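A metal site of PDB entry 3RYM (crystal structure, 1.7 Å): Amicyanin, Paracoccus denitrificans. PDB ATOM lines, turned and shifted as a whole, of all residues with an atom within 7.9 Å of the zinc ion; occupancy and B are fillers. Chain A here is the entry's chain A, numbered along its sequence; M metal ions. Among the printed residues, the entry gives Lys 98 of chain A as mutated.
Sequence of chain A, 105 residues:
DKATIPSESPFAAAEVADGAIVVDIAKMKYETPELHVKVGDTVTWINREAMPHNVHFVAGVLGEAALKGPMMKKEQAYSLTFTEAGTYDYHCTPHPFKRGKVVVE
A ring nitrogen (NE2) of His 53 sits close to the backbone carbonyl oxygen of Met 51 (3.3 Å).
SD of Met 51 lies within hydrogen-bond range of NE2 of His 95, 3.7 Å away.
The backbone NH (N) of Asn 54 sits close to the side-chain sulfur (SG) of Cys 92 (3.5 Å).
N of Cys 92 is in hydrogen-bond range of OH of Tyr 30, at 3.1 Å.
Four residues have an atom within 4 Å of the zinc ion: His 53, Cys 92, His 95 and Lys 98.
The nearest printed residue that does not touch the zinc ion is Pro 52 (4.4 Å).
ND1 of His 53 binds the zinc ion (2.1 Å).
NZ of Lys 98 is bound to the zinc ion (2.1 Å).
ND1 of His 95 is bound to the zinc ion, 2.1 Å away.
The zinc ion is bound by SG of Cys 92, 2.3 Å away.
The zinc ion has four donor atoms within binding distance.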
ATOM      1  N   ILE A  25       4.580  -9.737   4.395  1.00  0.00           N
ATOM      2  CA  ILE A  25       3.347 -10.279   3.836  1.00  0.00           C
ATOM      3  C   ILE A  25       3.714 -11.331   2.795  1.00  0.00           C
ATOM      4  O   ILE A  25       4.442 -11.055   1.850  1.00  0.00           O
ATOM      5  CB  ILE A  25       2.486  -9.217   3.193  1.00  0.00           C
ATOM      6  CG1 ILE A  25       2.259  -8.036   4.161  1.00  0.00           C
ATOM      7  CG2 ILE A  25       1.108  -9.797   2.802  1.00  0.00           C
ATOM      8  CD1 ILE A  25       1.465  -6.907   3.557  1.00  0.00           C
ATOM      9  N   ALA A  26       3.144 -12.496   3.044  1.00  0.00           N
ATOM     10  CA  ALA A  26       3.261 -13.632   2.174  1.00  0.00           C
ATOM     11  C   ALA A  26       1.890 -14.027   1.636  1.00  0.00           C
ATOM     12  O   ALA A  26       0.866 -13.589   2.078  1.00  0.00           O
ATOM     13  CB  ALA A  26       3.841 -14.802   2.959  1.00  0.00           C
ATOM     14  N   LYS A  27       1.908 -14.919   0.679  1.00  0.00           N
ATOM     15  CA  LYS A  27       0.658 -15.384   0.145  1.00  0.00           C
ATOM     16  C   LYS A  27      -0.263 -15.930   1.174  1.00  0.00           C
ATOM     17  O   LYS A  27      -1.390 -15.776   1.276  1.00  0.00           O
ATOM     18  CB  LYS A  27       0.903 -16.437  -0.934  1.00  0.00           C
ATOM     19  CG  LYS A  27      -0.350 -16.915  -1.548  1.00  0.00           C
ATOM     20  CD  LYS A  27      -0.225 -18.177  -2.499  1.00  0.00           C
ATOM     21  CE  LYS A  27      -1.531 -18.533  -3.144  1.00  0.00           C
ATOM     22  NZ  LYS A  27      -1.999 -17.640  -4.073  1.00  0.00           N
ATOM     23  N   MET A  28       0.272 -16.798   1.929  1.00  0.00           N
ATOM     24  CA  MET A  28      -0.616 -17.528   2.710  1.00  0.00           C
ATOM     25  C   MET A  28      -0.850 -16.974   4.099  1.00  0.00           C
ATOM     26  O   MET A  28      -1.570 -17.551   4.872  1.00  0.00           O
ATOM     27  CB  MET A  28      -0.024 -18.924   2.849  1.00  0.00           C
ATOM     28  CG  MET A  28      -0.003 -19.728   1.601  1.00  0.00           C
ATOM     29  SD  MET A  28      -1.646 -19.958   0.926  1.00  0.00           S
ATOM     30  CE  MET A  28      -2.386 -20.998   2.141  1.00  0.00           C
ATOM     31  N   LYS A  29      -0.124 -15.928   4.433  1.00  0.00           N
ATOM     32  CA  LYS A  29      -0.223 -15.349   5.752  1.00  0.00           C
ATOM     33  C   LYS A  29       0.616 -14.108   5.902  1.00  0.00           C
ATOM     34  O   LYS A  29       1.466 -13.861   5.135  1.00  0.00           O
ATOM     35  CB  LYS A  29       0.214 -16.356   6.818  1.00  0.00           C
ATOM     36  CG  LYS A  29       1.698 -16.824   6.693  1.00  0.00           C
ATOM     37  CD  LYS A  29       2.209 -17.339   8.044  1.00  0.00           C
ATOM     38  CE  LYS A  29       3.519 -18.076   7.901  1.00  0.00           C
ATOM     39  NZ  LYS A  29       3.854 -18.913   9.081  1.00  0.00           N
ATOM     40  N   TYR A  30       0.246 -13.261   6.860  1.00  0.00           N
ATOM     41  CA  TYR A  30       1.186 -12.307   7.377  1.00  0.00           C
ATOM     42  C   TYR A  30       2.159 -13.173   8.160  1.00  0.00           C
ATOM     43  O   TYR A  30       1.744 -14.020   8.953  1.00  0.00           O
ATOM     44  CB  TYR A  30       0.429 -11.315   8.304  1.00  0.00           C
ATOM     45  CG  TYR A  30      -0.558 -10.435   7.584  1.00  0.00           C
ATOM     46  CD1 TYR A  30      -0.130  -9.357   6.803  1.00  0.00           C
ATOM     47  CD2 TYR A  30      -1.929 -10.661   7.691  1.00  0.00           C
ATOM     48  CE1 TYR A  30      -1.036  -8.547   6.157  1.00  0.00           C
ATOM     49  CE2 TYR A  30      -2.832  -9.852   7.059  1.00  0.00           C
ATOM     50  CZ  TYR A  30      -2.395  -8.809   6.269  1.00  0.00           C
ATOM     51  OH  TYR A  30      -3.338  -8.026   5.649  1.00  0.00           O
ATOM     52  N   ASN A  47       5.433  -6.028   1.645  1.00  0.00           N
ATOM     53  CA  ASN A  47       4.944  -7.038   0.712  1.00  0.00           C
ATOM     54  C   ASN A  47       6.108  -7.753   0.015  1.00  0.00           C
ATOM     55  O   ASN A  47       6.896  -7.143  -0.705  1.00  0.00           O
ATOM     56  CB  ASN A  47       4.012  -6.433  -0.335  1.00  0.00           C
ATOM     57  CG  ASN A  47       3.347  -7.494  -1.187  1.00  0.00           C
ATOM     58  OD1 ASN A  47       3.547  -8.687  -0.932  1.00  0.00           O
ATOM     59  ND2 ASN A  47       2.562  -7.079  -2.154  1.00  0.00           N
ATOM     60  N   GLU A  49       5.587 -10.456  -2.014  1.00  0.00           N
ATOM     61  CA  GLU A  49       5.016 -11.146  -3.182  1.00  0.00           C
ATOM     62  C   GLU A  49       4.708 -10.153  -4.299  1.00  0.00           C
ATOM     63  O   GLU A  49       4.618  -8.990  -4.092  1.00  0.00           O
ATOM     64  CB  GLU A  49       3.690 -11.854  -2.863  1.00  0.00           C
ATOM     65  CG  GLU A  49       3.524 -12.663  -1.657  1.00  0.00           C
ATOM     66  CD  GLU A  49       4.243 -13.969  -1.719  1.00  0.00           C
ATOM     67  OE1 GLU A  49       4.862 -14.227  -2.702  1.00  0.00           O
ATOM     68  OE2 GLU A  49       4.226 -14.738  -0.784  1.00  0.00           O
ATOM     69  N   MET A  51       1.796 -10.261  -6.097  1.00  0.00           N
ATOM     70  CA  MET A  51       0.405  -9.959  -5.819  1.00  0.00           C
ATOM     71  C   MET A  51       0.308  -8.813  -4.822  1.00  0.00           C
ATOM     72  O   MET A  51       0.947  -8.889  -3.768  1.00  0.00           O
ATOM     73  CB  MET A  51      -0.275 -11.193  -5.227  1.00  0.00           C
ATOM     74  CG  MET A  51      -1.666 -10.941  -4.690  1.00  0.00           C
ATOM     75  SD  MET A  51      -2.897 -10.797  -5.964  1.00  0.00           S
ATOM     76  CE  MET A  51      -2.963 -12.476  -6.571  1.00  0.00           C
ATOM     77  N   PRO A  52      -0.467  -7.767  -5.135  1.00  0.00           N
ATOM     78  CA  PRO A  52      -0.599  -6.689  -4.156  1.00  0.00           C
ATOM     79  C   PRO A  52      -1.369  -7.125  -2.922  1.00  0.00           C
ATOM     80  O   PRO A  52      -2.317  -7.891  -3.021  1.00  0.00           O
ATOM     81  CB  PRO A  52      -1.375  -5.618  -4.904  1.00  0.00           C
ATOM     82  CG  PRO A  52      -1.164  -5.925  -6.365  1.00  0.00           C
ATOM     83  CD  PRO A  52      -1.096  -7.417  -6.419  1.00  0.00           C
ATOM     84  N   HIS A  53      -0.926  -6.626  -1.773  1.00  0.00           N
ATOM     85  CA  HIS A  53      -1.662  -6.838  -0.517  1.00  0.00           C
ATOM     86  C   HIS A  53      -1.742  -5.539   0.259  1.00  0.00           C
ATOM     87  O   HIS A  53      -1.060  -4.579  -0.062  1.00  0.00           O
ATOM     88  CB  HIS A  53      -0.918  -7.856   0.365  1.00  0.00           C
ATOM     89  CG  HIS A  53      -0.700  -9.181  -0.295  1.00  0.00           C
ATOM     90  ND1 HIS A  53      -1.682 -10.135  -0.381  1.00  0.00           N
ATOM     91  CD2 HIS A  53       0.389  -9.694  -0.924  1.00  0.00           C
ATOM     92  CE1 HIS A  53      -1.208 -11.212  -1.003  1.00  0.00           C
ATOM     93  NE2 HIS A  53       0.054 -10.965  -1.344  1.00  0.00           N
ATOM     94  N   ASN A  54      -2.530  -5.535   1.319  1.00  0.00           N
ATOM     95  CA  ASN A  54      -2.567  -4.367   2.195  1.00  0.00           C
ATOM     96  C   ASN A  54      -2.829  -4.776   3.620  1.00  0.00           C
ATOM     97  O   ASN A  54      -2.784  -5.964   3.942  1.00  0.00           O
ATOM     98  CB  ASN A  54      -3.558  -3.287   1.730  1.00  0.00           C
ATOM     99  CG  ASN A  54      -5.018  -3.670   2.021  1.00  0.00           C
ATOM    100  OD1 ASN A  54      -5.324  -4.865   2.143  1.00  0.00           O
ATOM    101  ND2 ASN A  54      -5.904  -2.691   2.087  1.00  0.00           N
ATOM    102  N   VAL A  55      -3.050  -3.791   4.473  1.00  0.00           N
ATOM    103  CA  VAL A  55      -3.570  -4.028   5.821  1.00  0.00           C
ATOM    104  C   VAL A  55      -4.789  -3.166   6.001  1.00  0.00           C
ATOM    105  O   VAL A  55      -4.803  -1.995   5.582  1.00  0.00           O
ATOM    106  CB  VAL A  55      -2.526  -3.762   6.949  1.00  0.00           C
ATOM    107  CG1 VAL A  55      -1.375  -4.755   6.873  1.00  0.00           C
ATOM    108  CG2 VAL A  55      -2.029  -2.321   6.892  1.00  0.00           C
ATOM    109  N   MET A  71      -2.778  -0.167  -1.266  1.00  0.00           N
ATOM    110  CA  MET A  71      -2.305  -1.436  -1.773  1.00  0.00           C
ATOM    111  C   MET A  71      -0.803  -1.383  -2.025  1.00  0.00           C
ATOM    112  O   MET A  71      -0.290  -0.446  -2.584  1.00  0.00           O
ATOM    113  CB  MET A  71      -3.050  -1.780  -3.059  1.00  0.00           C
ATOM    114  CG  MET A  71      -4.548  -2.037  -2.826  1.00  0.00           C
ATOM    115  SD  MET A  71      -4.899  -3.412  -1.700  1.00  0.00           S
ATOM    116  CE  MET A  71      -4.293  -4.818  -2.589  1.00  0.00           C
ATOM    117  N   HIS A  91      -6.902  -7.219   8.364  1.00  0.00           N
ATOM    118  CA  HIS A  91      -6.890  -8.230   7.293  1.00  0.00           C
ATOM    119  C   HIS A  91      -6.496  -7.609   5.987  1.00  0.00           C
ATOM    120  O   HIS A  91      -6.314  -6.391   5.871  1.00  0.00           O
ATOM    121  CB  HIS A  91      -8.273  -8.887   7.170  1.00  0.00           C
ATOM    122  CG  HIS A  91      -9.331  -7.955   6.653  1.00  0.00           C
ATOM    123  ND1 HIS A  91     -10.063  -7.141   7.481  1.00  0.00           N
ATOM    124  CD2 HIS A  91      -9.752  -7.684   5.400  1.00  0.00           C
ATOM    125  CE1 HIS A  91     -10.906  -6.424   6.767  1.00  0.00           C
ATOM    126  NE2 HIS A  91     -10.732  -6.740   5.487  1.00  0.00           N
ATOM    127  N   CYS A  92      -6.355  -8.441   4.956  1.00  0.00           N
ATOM    128  CA  CYS A  92      -6.009  -7.952   3.615  1.00  0.00           C
ATOM    129  C   CYS A  92      -7.269  -7.761   2.791  1.00  0.00           C
ATOM    130  O   CYS A  92      -8.044  -8.696   2.578  1.00  0.00           O
ATOM    131  CB  CYS A  92      -5.089  -8.967   2.936  1.00  0.00           C
ATOM    132  SG  CYS A  92      -4.520  -8.399   1.361  1.00  0.00           S
ATOM    133  N   THR A  93      -7.482  -6.548   2.296  1.00  0.00           N
ATOM    134  CA  THR A  93      -8.775  -6.226   1.684  1.00  0.00           C
ATOM    135  C   THR A  93      -9.215  -7.170   0.565  1.00  0.00           C
ATOM    136  O   THR A  93     -10.331  -7.686   0.568  1.00  0.00           O
ATOM    137  CB  THR A  93      -8.810  -4.761   1.220  1.00  0.00           C
ATOM    138  OG1 THR A  93      -8.566  -3.900   2.324  1.00  0.00           O
ATOM    139  CG2 THR A  93     -10.173  -4.430   0.599  1.00  0.00           C
ATOM    140  N   PRO A  94      -8.331  -7.402  -0.422  1.00  0.00           N
ATOM    141  CA  PRO A  94      -8.721  -8.301  -1.527  1.00  0.00           C
ATOM    142  C   PRO A  94      -8.698  -9.763  -1.133  1.00  0.00           C
ATOM    143  O   PRO A  94      -9.300 -10.592  -1.847  1.00  0.00           O
ATOM    144  CB  PRO A  94      -7.648  -8.036  -2.572  1.00  0.00           C
ATOM    145  CG  PRO A  94      -6.476  -7.529  -1.803  1.00  0.00           C
ATOM    146  CD  PRO A  94      -7.065  -6.724  -0.678  1.00  0.00           C
ATOM    147  N   HIS A  95      -8.011 -10.106  -0.051  1.00  0.00           N
ATOM    148  CA  HIS A  95      -7.892 -11.495   0.408  1.00  0.00           C
ATOM    149  C   HIS A  95      -8.241 -11.533   1.894  1.00  0.00           C
ATOM    150  O   HIS A  95      -7.373 -11.819   2.724  1.00  0.00           O
ATOM    151  CB  HIS A  95      -6.462 -11.992   0.204  1.00  0.00           C
ATOM    152  CG  HIS A  95      -5.875 -11.626  -1.130  1.00  0.00           C
ATOM    153  ND1 HIS A  95      -4.681 -10.962  -1.247  1.00  0.00           N
ATOM    154  CD2 HIS A  95      -6.328 -11.822  -2.394  1.00  0.00           C
ATOM    155  CE1 HIS A  95      -4.413 -10.739  -2.522  1.00  0.00           C
ATOM    156  NE2 HIS A  95      -5.399 -11.264  -3.249  1.00  0.00           N
ATOM    157  N   PRO A  96      -9.509 -11.283   2.227  1.00  0.00           N
ATOM    158  CA  PRO A  96      -9.946 -10.974   3.598  1.00  0.00           C
ATOM    159  C   PRO A  96      -9.865 -12.099   4.578  1.00  0.00           C
ATOM    160  O   PRO A  96      -9.978 -11.957   5.764  1.00  0.00           O
ATOM    161  CB  PRO A  96     -11.390 -10.525   3.410  1.00  0.00           C
ATOM    162  CG  PRO A  96     -11.835 -11.184   2.154  1.00  0.00           C
ATOM    163  CD  PRO A  96     -10.620 -11.181   1.258  1.00  0.00           C
ATOM    164  N   PHE A  97      -9.947 -13.266   4.038  1.00  0.00           N
ATOM    165  CA  PHE A  97      -9.548 -14.362   4.830  1.00  0.00           C
ATOM    166  C   PHE A  97      -8.064 -14.321   5.349  1.00  0.00           C
ATOM    167  O   PHE A  97      -7.721 -14.983   6.236  1.00  0.00           O
ATOM    168  CB  PHE A  97      -9.767 -15.653   4.023  1.00  0.00           C
ATOM    169  CG  PHE A  97      -8.999 -15.665   2.718  1.00  0.00           C
ATOM    170  CD1 PHE A  97      -7.713 -16.137   2.658  1.00  0.00           C
ATOM    171  CD2 PHE A  97      -9.579 -15.203   1.551  1.00  0.00           C
ATOM    172  CE1 PHE A  97      -7.008 -16.153   1.460  1.00  0.00           C
ATOM    173  CE2 PHE A  97      -8.868 -15.225   0.359  1.00  0.00           C
ATOM    174  CZ  PHE A  97      -7.590 -15.690   0.331  1.00  0.00           C
ATOM    175  N   LYS A  98      -7.123 -13.522   4.927  1.00  0.00           N
ATOM    176  CA  LYS A  98      -5.769 -13.407   5.541  1.00  0.00           C
ATOM    177  C   LYS A  98      -5.836 -12.324   6.583  1.00  0.00           C
ATOM    178  O   LYS A  98      -6.118 -11.185   6.353  1.00  0.00           O
ATOM    179  CB  LYS A  98      -4.801 -13.000   4.413  1.00  0.00           C
ATOM    180  CG  LYS A  98      -3.345 -12.856   4.857  1.00  0.00           C
ATOM    181  CD  LYS A  98      -2.370 -12.901   3.714  1.00  0.00           C
ATOM    182  CE  LYS A  98      -2.473 -11.704   2.776  1.00  0.00           C
ATOM    183  NZ  LYS A  98      -3.488 -11.945   1.713  1.00  0.00           N
HETATM  184 ZN    ZN M   1      -3.557 -10.310   0.446  1.00  0.00          ZN
